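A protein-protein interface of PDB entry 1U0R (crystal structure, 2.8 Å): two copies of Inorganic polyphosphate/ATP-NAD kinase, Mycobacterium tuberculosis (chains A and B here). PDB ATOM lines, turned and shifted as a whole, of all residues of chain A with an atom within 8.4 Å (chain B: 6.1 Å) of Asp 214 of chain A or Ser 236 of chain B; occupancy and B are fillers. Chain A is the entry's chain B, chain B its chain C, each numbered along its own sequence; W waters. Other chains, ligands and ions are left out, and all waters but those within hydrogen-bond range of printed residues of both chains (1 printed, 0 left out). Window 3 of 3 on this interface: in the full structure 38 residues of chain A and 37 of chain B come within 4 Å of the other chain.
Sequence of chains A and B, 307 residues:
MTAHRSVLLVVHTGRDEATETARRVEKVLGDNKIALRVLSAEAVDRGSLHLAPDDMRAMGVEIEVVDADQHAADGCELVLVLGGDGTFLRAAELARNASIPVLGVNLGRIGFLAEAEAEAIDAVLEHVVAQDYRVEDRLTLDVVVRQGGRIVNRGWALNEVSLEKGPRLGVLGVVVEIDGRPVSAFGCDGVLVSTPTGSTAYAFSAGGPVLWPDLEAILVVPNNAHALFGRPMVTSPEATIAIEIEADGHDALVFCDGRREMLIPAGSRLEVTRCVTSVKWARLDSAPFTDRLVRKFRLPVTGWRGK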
ATOM      1  N   GLU A 136      -5.953   1.780 -20.337  1.00  0.00           N
ATOM      2  CA  GLU A 136      -6.443   0.709 -21.209  1.00  0.00           C
ATOM      3  C   GLU A 136      -5.692   0.544 -22.542  1.00  0.00           C
ATOM      4  O   GLU A 136      -5.567   1.486 -23.319  1.00  0.00           O
ATOM      5  CB  GLU A 136      -7.975   0.762 -21.385  1.00  0.00           C
ATOM      6  CG  GLU A 136      -8.517   1.927 -22.196  1.00  0.00           C
ATOM      7  CD  GLU A 136      -9.843   1.585 -22.865  1.00  0.00           C
ATOM      8  OE1 GLU A 136      -9.821   0.908 -23.934  1.00  0.00           O
ATOM      9  OE2 GLU A 136     -10.909   1.983 -22.317  1.00  0.00           O
ATOM     10  N   ASP A 137      -5.177  -0.666 -22.767  1.00  0.00           N
ATOM     11  CA  ASP A 137      -4.585  -1.086 -24.042  1.00  0.00           C
ATOM     12  C   ASP A 137      -5.586  -0.904 -25.220  1.00  0.00           C
ATOM     13  O   ASP A 137      -6.767  -1.261 -25.094  1.00  0.00           O
ATOM     14  CB  ASP A 137      -4.164  -2.564 -23.923  1.00  0.00           C
ATOM     15  CG  ASP A 137      -2.639  -2.779 -24.051  1.00  0.00           C
ATOM     16  OD1 ASP A 137      -1.836  -1.877 -23.677  1.00  0.00           O
ATOM     17  OD2 ASP A 137      -2.159  -3.848 -24.512  1.00  0.00           O
ATOM     18  N   ARG A 138      -5.124  -0.353 -26.348  1.00  0.00           N
ATOM     19  CA  ARG A 138      -6.000  -0.148 -27.514  1.00  0.00           C
ATOM     20  C   ARG A 138      -5.411  -0.636 -28.844  1.00  0.00           C
ATOM     21  O   ARG A 138      -4.246  -0.361 -29.164  1.00  0.00           O
ATOM     22  CB  ARG A 138      -6.434   1.319 -27.624  1.00  0.00           C
ATOM     23  CG  ARG A 138      -7.524   1.604 -28.663  1.00  0.00           C
ATOM     24  CD  ARG A 138      -8.964   1.620 -28.144  1.00  0.00           C
ATOM     25  NE  ARG A 138      -9.175   2.423 -26.931  1.00  0.00           N
ATOM     26  CZ  ARG A 138      -9.635   3.682 -26.887  1.00  0.00           C
ATOM     27  NH1 ARG A 138      -9.938   4.354 -28.001  1.00  0.00           N
ATOM     28  NH2 ARG A 138      -9.789   4.280 -25.706  1.00  0.00           N
ATOM     29  N   LEU A 139      -6.249  -1.336 -29.610  1.00  0.00           N
ATOM     30  CA  LEU A 139      -5.900  -1.942 -30.900  1.00  0.00           C
ATOM     31  C   LEU A 139      -5.035  -1.060 -31.750  1.00  0.00           C
ATOM     32  O   LEU A 139      -5.403   0.062 -32.129  1.00  0.00           O
ATOM     33  CB  LEU A 139      -7.178  -2.298 -31.673  1.00  0.00           C
ATOM     34  CG  LEU A 139      -7.313  -3.052 -33.002  1.00  0.00           C
ATOM     35  CD1 LEU A 139      -6.045  -3.238 -33.763  1.00  0.00           C
ATOM     36  CD2 LEU A 139      -7.945  -4.387 -32.742  1.00  0.00           C
ATOM     37  N   PRO A 196     -10.795   1.079 -35.325  1.00  0.00           N
ATOM     38  CA  PRO A 196     -12.043   1.717 -34.898  1.00  0.00           C
ATOM     39  C   PRO A 196     -11.896   3.152 -34.371  1.00  0.00           C
ATOM     40  O   PRO A 196     -12.818   3.974 -34.458  1.00  0.00           O
ATOM     41  CB  PRO A 196     -12.552   0.778 -33.808  1.00  0.00           C
ATOM     42  CG  PRO A 196     -12.024  -0.550 -34.216  1.00  0.00           C
ATOM     43  CD  PRO A 196     -10.624  -0.232 -34.669  1.00  0.00           C
ATOM     44  N   THR A 197     -10.743   3.480 -33.825  1.00  0.00           N
ATOM     45  CA  THR A 197     -10.535   4.849 -33.379  1.00  0.00           C
ATOM     46  C   THR A 197     -10.458   5.734 -34.627  1.00  0.00           C
ATOM     47  O   THR A 197     -10.968   6.858 -34.632  1.00  0.00           O
ATOM     48  CB  THR A 197      -9.269   4.941 -32.476  1.00  0.00           C
ATOM     49  OG1 THR A 197      -9.179   3.759 -31.656  1.00  0.00           O
ATOM     50  CG2 THR A 197      -9.458   5.997 -31.426  1.00  0.00           C
ATOM     51  N   VAL A 210     -19.054   4.241 -39.046  1.00  0.00           N
ATOM     52  CA  VAL A 210     -18.382   4.659 -37.830  1.00  0.00           C
ATOM     53  C   VAL A 210     -18.346   3.500 -36.870  1.00  0.00           C
ATOM     54  O   VAL A 210     -19.360   2.847 -36.609  1.00  0.00           O
ATOM     55  CB  VAL A 210     -18.961   5.937 -37.200  1.00  0.00           C
ATOM     56  CG1 VAL A 210     -20.396   6.158 -37.598  1.00  0.00           C
ATOM     57  CG2 VAL A 210     -18.848   5.913 -35.705  1.00  0.00           C
ATOM     58  N   LEU A 211     -17.153   3.226 -36.361  1.00  0.00           N
ATOM     59  CA  LEU A 211     -16.942   2.115 -35.460  1.00  0.00           C
ATOM     60  C   LEU A 211     -16.751   2.697 -34.105  1.00  0.00           C
ATOM     61  O   LEU A 211     -15.881   3.540 -33.965  1.00  0.00           O
ATOM     62  CB  LEU A 211     -15.689   1.334 -35.866  1.00  0.00           C
ATOM     63  CG  LEU A 211     -15.926   0.242 -36.918  1.00  0.00           C
ATOM     64  CD1 LEU A 211     -16.699   0.784 -38.108  1.00  0.00           C
ATOM     65  CD2 LEU A 211     -14.633  -0.356 -37.385  1.00  0.00           C
ATOM     66  N   TRP A 212     -17.556   2.281 -33.119  1.00  0.00           N
ATOM     67  CA  TRP A 212     -17.334   2.623 -31.707  1.00  0.00           C
ATOM     68  C   TRP A 212     -15.956   2.139 -31.243  1.00  0.00           C
ATOM     69  O   TRP A 212     -15.520   1.081 -31.701  1.00  0.00           O
ATOM     70  CB  TRP A 212     -18.447   2.035 -30.866  1.00  0.00           C
ATOM     71  CG  TRP A 212     -19.575   2.996 -30.658  1.00  0.00           C
ATOM     72  CD1 TRP A 212     -19.963   3.542 -29.485  1.00  0.00           C
ATOM     73  CD2 TRP A 212     -20.449   3.557 -31.663  1.00  0.00           C
ATOM     74  NE1 TRP A 212     -21.030   4.389 -29.684  1.00  0.00           N
ATOM     75  CE2 TRP A 212     -21.332   4.429 -31.012  1.00  0.00           C
ATOM     76  CE3 TRP A 212     -20.553   3.426 -33.060  1.00  0.00           C
ATOM     77  CZ2 TRP A 212     -22.309   5.141 -31.690  1.00  0.00           C
ATOM     78  CZ3 TRP A 212     -21.544   4.135 -33.734  1.00  0.00           C
ATOM     79  CH2 TRP A 212     -22.403   4.969 -33.058  1.00  0.00           C
ATOM     80  N   PRO A 213     -15.279   2.885 -30.347  1.00  0.00           N
ATOM     81  CA  PRO A 213     -13.822   2.776 -30.146  1.00  0.00           C
ATOM     82  C   PRO A 213     -13.375   1.568 -29.353  1.00  0.00           C
ATOM     83  O   PRO A 213     -12.191   1.191 -29.374  1.00  0.00           O
ATOM     84  CB  PRO A 213     -13.483   4.016 -29.330  1.00  0.00           C
ATOM     85  CG  PRO A 213     -14.711   4.775 -29.212  1.00  0.00           C
ATOM     86  CD  PRO A 213     -15.853   3.847 -29.404  1.00  0.00           C
ATOM     87  N   ASP A 214     -14.329   0.948 -28.676  1.00  0.00           N
ATOM     88  CA  ASP A 214     -14.040  -0.225 -27.872  1.00  0.00           C
ATOM     89  C   ASP A 214     -14.300  -1.481 -28.618  1.00  0.00           C
ATOM     90  O   ASP A 214     -14.278  -2.547 -28.027  1.00  0.00           O
ATOM     91  CB  ASP A 214     -14.885  -0.235 -26.604  1.00  0.00           C
ATOM     92  CG  ASP A 214     -16.347  -0.297 -26.899  1.00  0.00           C
ATOM     93  OD1 ASP A 214     -16.897  -1.363 -26.679  1.00  0.00           O
ATOM     94  OD2 ASP A 214     -17.032   0.641 -27.345  1.00  0.00           O
ATOM     95  N   LEU A 215     -14.559  -1.395 -29.908  1.00  0.00           N
ATOM     96  CA  LEU A 215     -14.734  -2.625 -30.649  1.00  0.00           C
ATOM     97  C   LEU A 215     -13.360  -3.074 -31.094  1.00  0.00           C
ATOM     98  O   LEU A 215     -12.453  -2.264 -31.191  1.00  0.00           O
ATOM     99  CB  LEU A 215     -15.676  -2.407 -31.825  1.00  0.00           C
ATOM    100  CG  LEU A 215     -15.501  -3.249 -33.077  1.00  0.00           C
ATOM    101  CD1 LEU A 215     -16.327  -4.482 -33.009  1.00  0.00           C
ATOM    102  CD2 LEU A 215     -15.863  -2.422 -34.251  1.00  0.00           C
ATOM    103  N   GLU A 216     -13.187  -4.361 -31.337  1.00  0.00           N
ATOM    104  CA  GLU A 216     -11.980  -4.811 -31.990  1.00  0.00           C
ATOM    105  C   GLU A 216     -12.246  -5.279 -33.409  1.00  0.00           C
ATOM    106  O   GLU A 216     -12.803  -6.349 -33.645  1.00  0.00           O
ATOM    107  CB  GLU A 216     -11.387  -5.949 -31.212  1.00  0.00           C
ATOM    108  CG  GLU A 216     -11.446  -5.767 -29.713  1.00  0.00           C
ATOM    109  CD  GLU A 216     -10.077  -5.905 -29.131  1.00  0.00           C
ATOM    110  OE1 GLU A 216      -9.509  -4.860 -28.725  1.00  0.00           O
ATOM    111  OE2 GLU A 216      -9.578  -7.059 -29.140  1.00  0.00           O
ATOM    112  N   ALA A 217     -11.845  -4.475 -34.376  1.00  0.00           N
ATOM    113  CA  ALA A 217     -11.996  -4.865 -35.756  1.00  0.00           C
ATOM    114  C   ALA A 217     -11.003  -4.080 -36.562  1.00  0.00           C
ATOM    115  O   ALA A 217     -10.475  -3.084 -36.101  1.00  0.00           O
ATOM    116  CB  ALA A 217     -13.367  -4.595 -36.207  1.00  0.00           C
ATOM    117  N   ARG A 283      -7.493   6.750 -19.172  1.00  0.00           N
ATOM    118  CA  ARG A 283      -8.951   6.863 -19.258  1.00  0.00           C
ATOM    119  C   ARG A 283      -9.505   7.582 -18.045  1.00  0.00           C
ATOM    120  O   ARG A 283      -9.036   7.354 -16.938  1.00  0.00           O
ATOM    121  CB  ARG A 283      -9.602   5.480 -19.386  1.00  0.00           C
ATOM    122  CG  ARG A 283      -9.985   5.110 -20.818  1.00  0.00           C
ATOM    123  CD  ARG A 283     -11.475   4.845 -21.015  1.00  0.00           C
ATOM    124  NE  ARG A 283     -11.948   5.379 -22.293  1.00  0.00           N
ATOM    125  CZ  ARG A 283     -13.035   6.139 -22.444  1.00  0.00           C
ATOM    126  NH1 ARG A 283     -13.788   6.465 -21.392  1.00  0.00           N
ATOM    127  NH2 ARG A 283     -13.373   6.578 -23.656  1.00  0.00           N
ATOM    128  N   PHE A 289     -18.072   7.756 -26.129  1.00  0.00           N
ATOM    129  CA  PHE A 289     -17.863   7.955 -27.552  1.00  0.00           C
ATOM    130  C   PHE A 289     -19.105   8.484 -28.242  1.00  0.00           C
ATOM    131  O   PHE A 289     -19.025   9.446 -29.010  1.00  0.00           O
ATOM    132  CB  PHE A 289     -17.462   6.671 -28.227  1.00  0.00           C
ATOM    133  CG  PHE A 289     -17.430   6.775 -29.693  1.00  0.00           C
ATOM    134  CD1 PHE A 289     -16.378   7.411 -30.324  1.00  0.00           C
ATOM    135  CD2 PHE A 289     -18.448   6.274 -30.442  1.00  0.00           C
ATOM    136  CE1 PHE A 289     -16.318   7.520 -31.673  1.00  0.00           C
ATOM    137  CE2 PHE A 289     -18.414   6.378 -31.805  1.00  0.00           C
ATOM    138  CZ  PHE A 289     -17.337   7.000 -32.424  1.00  0.00           C
ATOM    139  N   THR A 290     -20.249   7.866 -27.974  1.00  0.00           N
ATOM    140  CA  THR A 290     -21.498   8.327 -28.538  1.00  0.00           C
ATOM    141  C   THR A 290     -21.702   9.805 -28.406  1.00  0.00           C
ATOM    142  O   THR A 290     -22.227  10.409 -29.304  1.00  0.00           O
ATOM    143  CB  THR A 290     -22.656   7.600 -27.916  1.00  0.00           C
ATOM    144  OG1 THR A 290     -22.371   6.195 -27.940  1.00  0.00           O
ATOM    145  CG2 THR A 290     -23.915   7.710 -28.791  1.00  0.00           C
ATOM    146  N   ASP B 179     -25.795   2.240 -26.339  1.00  0.00           N
ATOM    147  CA  ASP B 179     -25.241   2.152 -25.028  1.00  0.00           C
ATOM    148  C   ASP B 179     -25.792   3.204 -24.091  1.00  0.00           C
ATOM    149  O   ASP B 179     -25.107   3.708 -23.224  1.00  0.00           O
ATOM    150  CB  ASP B 179     -23.719   2.125 -25.094  1.00  0.00           C
ATOM    151  CG  ASP B 179     -23.177   0.716 -25.335  1.00  0.00           C
ATOM    152  OD1 ASP B 179     -23.867  -0.290 -25.001  1.00  0.00           O
ATOM    153  OD2 ASP B 179     -22.054   0.508 -25.852  1.00  0.00           O
ATOM    154  N   GLU B 216     -17.070 -10.638 -34.284  1.00  0.00           N
ATOM    155  CA  GLU B 216     -18.202 -10.465 -33.422  1.00  0.00           C
ATOM    156  C   GLU B 216     -18.354  -8.985 -33.228  1.00  0.00           C
ATOM    157  O   GLU B 216     -17.539  -8.329 -32.574  1.00  0.00           O
ATOM    158  CB  GLU B 216     -17.943 -11.099 -32.087  1.00  0.00           C
ATOM    159  CG  GLU B 216     -17.000 -12.276 -32.106  1.00  0.00           C
ATOM    160  CD  GLU B 216     -17.442 -13.370 -31.152  1.00  0.00           C
ATOM    161  OE1 GLU B 216     -16.884 -14.488 -31.248  1.00  0.00           O
ATOM    162  OE2 GLU B 216     -18.344 -13.127 -30.310  1.00  0.00           O
ATOM    163  N   ALA B 217     -19.391  -8.449 -33.836  1.00  0.00           N
ATOM    164  CA  ALA B 217     -19.709  -7.048 -33.723  1.00  0.00           C
ATOM    165  C   ALA B 217     -21.189  -6.942 -34.020  1.00  0.00           C
ATOM    166  O   ALA B 217     -21.836  -7.951 -34.306  1.00  0.00           O
ATOM    167  CB  ALA B 217     -18.898  -6.245 -34.708  1.00  0.00           C
ATOM    168  N   ILE B 218     -21.734  -5.732 -33.939  1.00  0.00           N
ATOM    169  CA  ILE B 218     -23.130  -5.507 -34.273  1.00  0.00           C
ATOM    170  C   ILE B 218     -23.193  -4.352 -35.247  1.00  0.00           C
ATOM    171  O   ILE B 218     -22.521  -3.351 -35.064  1.00  0.00           O
ATOM    172  CB  ILE B 218     -23.938  -5.206 -33.004  1.00  0.00           C
ATOM    173  CG1 ILE B 218     -24.184  -6.490 -32.207  1.00  0.00           C
ATOM    174  CG2 ILE B 218     -25.265  -4.533 -33.344  1.00  0.00           C
ATOM    175  CD1 ILE B 218     -24.709  -6.269 -30.815  1.00  0.00           C
ATOM    176  N   VAL B 234     -21.002   0.530 -36.528  1.00  0.00           N
ATOM    177  CA  VAL B 234     -20.635  -0.824 -36.099  1.00  0.00           C
ATOM    178  C   VAL B 234     -20.123  -0.759 -34.705  1.00  0.00           C
ATOM    179  O   VAL B 234     -19.387   0.154 -34.338  1.00  0.00           O
ATOM    180  CB  VAL B 234     -19.555  -1.443 -36.929  1.00  0.00           C
ATOM    181  CG1 VAL B 234     -19.309  -2.862 -36.467  1.00  0.00           C
ATOM    182  CG2 VAL B 234     -19.973  -1.446 -38.375  1.00  0.00           C
ATOM    183  N   THR B 235     -20.475  -1.778 -33.947  1.00  0.00           N
ATOM    184  CA  THR B 235     -20.539  -1.725 -32.490  1.00  0.00           C
ATOM    185  C   THR B 235     -19.992  -3.027 -31.999  1.00  0.00           C
ATOM    186  O   THR B 235     -19.961  -3.980 -32.757  1.00  0.00           O
ATOM    187  CB  THR B 235     -22.006  -1.546 -32.153  1.00  0.00           C
ATOM    188  OG1 THR B 235     -22.171  -0.275 -31.534  1.00  0.00           O
ATOM    189  CG2 THR B 235     -22.511  -2.515 -31.161  1.00  0.00           C
ATOM    190  N   SER B 236     -19.509  -3.082 -30.768  1.00  0.00           N
ATOM    191  CA  SER B 236     -18.870  -4.304 -30.294  1.00  0.00           C
ATOM    192  C   SER B 236     -19.993  -5.251 -29.925  1.00  0.00           C
ATOM    193  O   SER B 236     -21.131  -4.845 -29.858  1.00  0.00           O
ATOM    194  CB  SER B 236     -18.047  -3.999 -29.070  1.00  0.00           C
ATOM    195  OG  SER B 236     -18.954  -3.653 -28.059  1.00  0.00           O
ATOM    196  N   PRO B 237     -19.704  -6.497 -29.622  1.00  0.00           N
ATOM    197  CA  PRO B 237     -20.788  -7.445 -29.421  1.00  0.00           C
ATOM    198  C   PRO B 237     -21.544  -7.194 -28.104  1.00  0.00           C
ATOM    199  O   PRO B 237     -22.665  -7.669 -27.978  1.00  0.00           O
ATOM    200  CB  PRO B 237     -20.060  -8.782 -29.410  1.00  0.00           C
ATOM    201  CG  PRO B 237     -18.651  -8.486 -29.770  1.00  0.00           C
ATOM    202  CD  PRO B 237     -18.388  -7.102 -29.374  1.00  0.00           C
ATOM    203  N   GLU B 238     -20.939  -6.446 -27.175  1.00  0.00           N
ATOM    204  CA  GLU B 238     -21.504  -6.154 -25.860  1.00  0.00           C
ATOM    205  C   GLU B 238     -22.376  -4.898 -25.791  1.00  0.00           C
ATOM    206  O   GLU B 238     -22.681  -4.420 -24.698  1.00  0.00           O
ATOM    207  CB  GLU B 238     -20.404  -5.974 -24.818  1.00  0.00           C
ATOM    208  CG  GLU B 238     -19.436  -7.129 -24.662  1.00  0.00           C
ATOM    209  CD  GLU B 238     -18.181  -6.924 -25.511  1.00  0.00           C
ATOM    210  OE1 GLU B 238     -17.848  -5.731 -25.794  1.00  0.00           O
ATOM    211  OE2 GLU B 238     -17.537  -7.938 -25.926  1.00  0.00           O
ATOM    212  N   ALA B 239     -22.778  -4.333 -26.919  1.00  0.00           N
ATOM    213  CA  ALA B 239     -23.471  -3.059 -26.845  1.00  0.00           C
ATOM    214  C   ALA B 239     -24.931  -3.322 -26.863  1.00  0.00           C
ATOM    215  O   ALA B 239     -25.342  -4.380 -27.271  1.00  0.00           O
ATOM    216  CB  ALA B 239     -23.096  -2.194 -27.998  1.00  0.00           C
HETATM  217  O   HOH W   1     -19.241  -0.848 -28.831  1.00  0.00           O
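The backbone NH (N) of Val 234 of chain B lies within hydrogen-bond range of the backbone carbonyl oxygen (O) of Val 210 of chain A (2.8 Å).
N of Trp 212 of chain A is in hydrogen-bond range of O of Val 234 of chain B, at 3.1 Å.
The side-chain carboxylate of Asp 214 of chain A sits at hydrogen-bond distance from the side-chain hydroxyl of Ser 236 of chain B (3.4 Å).
The side-chain hydroxyl (OG) of Ser 236 of chain B lies within hydrogen-bond range of the side-chain carboxylate (OE1) of Glu 238 of chain B, 3.3 Å away.
The backbone carbonyl oxygen (O) of Thr 235 of chain B lies within hydrogen-bond range of the backbone NH (N) of Ile 218 of chain B (2.8 Å).
The indole nitrogen of Trp 212 of chain A sits at hydrogen-bond distance from the side-chain hydroxyl of Thr 290 of chain A (2.8 Å).
Among the printed residues, pairs that only touch across the chains: Leu 211 of chain A with Val 234 of chain B (3.3 Å), Leu 215 of chain A with Ala 217 of chain B (3.6 Å), Leu 215 of chain A with Thr 235 of chain B (3.7 Å) and Leu 215 of chain A with Ser 236 of chain B (3.7 Å).
Thr 197 of chain A touches none of the printed residues of chain B.
Printed residues of chain B within 4 Å of Val 210 of chain A: Val 234 (2.8 Å).
Of the printed residues of chain B, Trp 212 of chain A touches Val 234 (3.1 Å).
Asp 214 of chain A touches one residue of chain B.
Asp 179 of chain B touches none of the printed residues of chain A.
Of the printed residues of chain A, Ala 217 of chain B touches Leu 215.
Of the printed residues of chain A, Val 234 of chain B touches Val 210, Leu 211 and Trp 212.
Of chain A, only Leu 215 comes within 4 Å of Thr 235 of chain B.
Ser 236 of chain B touches just these residues of chain A: Asp 214 (3.4 Å) and Leu 215 (3.7 Å).
No residue of chain A comes within 4 Å of Pro 237 of chain B.
The nearest residue of chain B that does not touch Asp 214 of chain A is Glu 238 of chain B (4.6 Å).
Hydrophobic or aromatic side chains of chain A within 4 Å of the printed part of chain B: Leu 211, Trp 212 and Leu 215.
Along chain A the printed residues that touch a printed residue of chain B span positions 210 to 215.
Of the 10 printed residues of chain B, 4 touch a printed residue of chain A.
Printed residues of chain B that touch a printed residue of chain A: Ala 217, Val 234, Thr 235 and Ser 236.
Hydrophobic or aromatic side chains of chain B that line the printed part of chain A: Ala 217 and Val 234.
Among the printed residues, 7 pairs touch across the chains.
Among the printed residues, no Asp or Glu carboxylate lies within 4 Å of a Lys or Arg side-chain nitrogen of the other chain.
Positions printed for both chains: 216 and 217.
Of the 7 pairs that touch across the chains among the printed residues, none has its exchanged pair printed and touching as well.
Water W1 bridges the side-chain hydroxyl of Ser 236 of chain B (2.9 Å) and the side-chain carboxylate of Asp 214 of chain A (3.1 Å).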
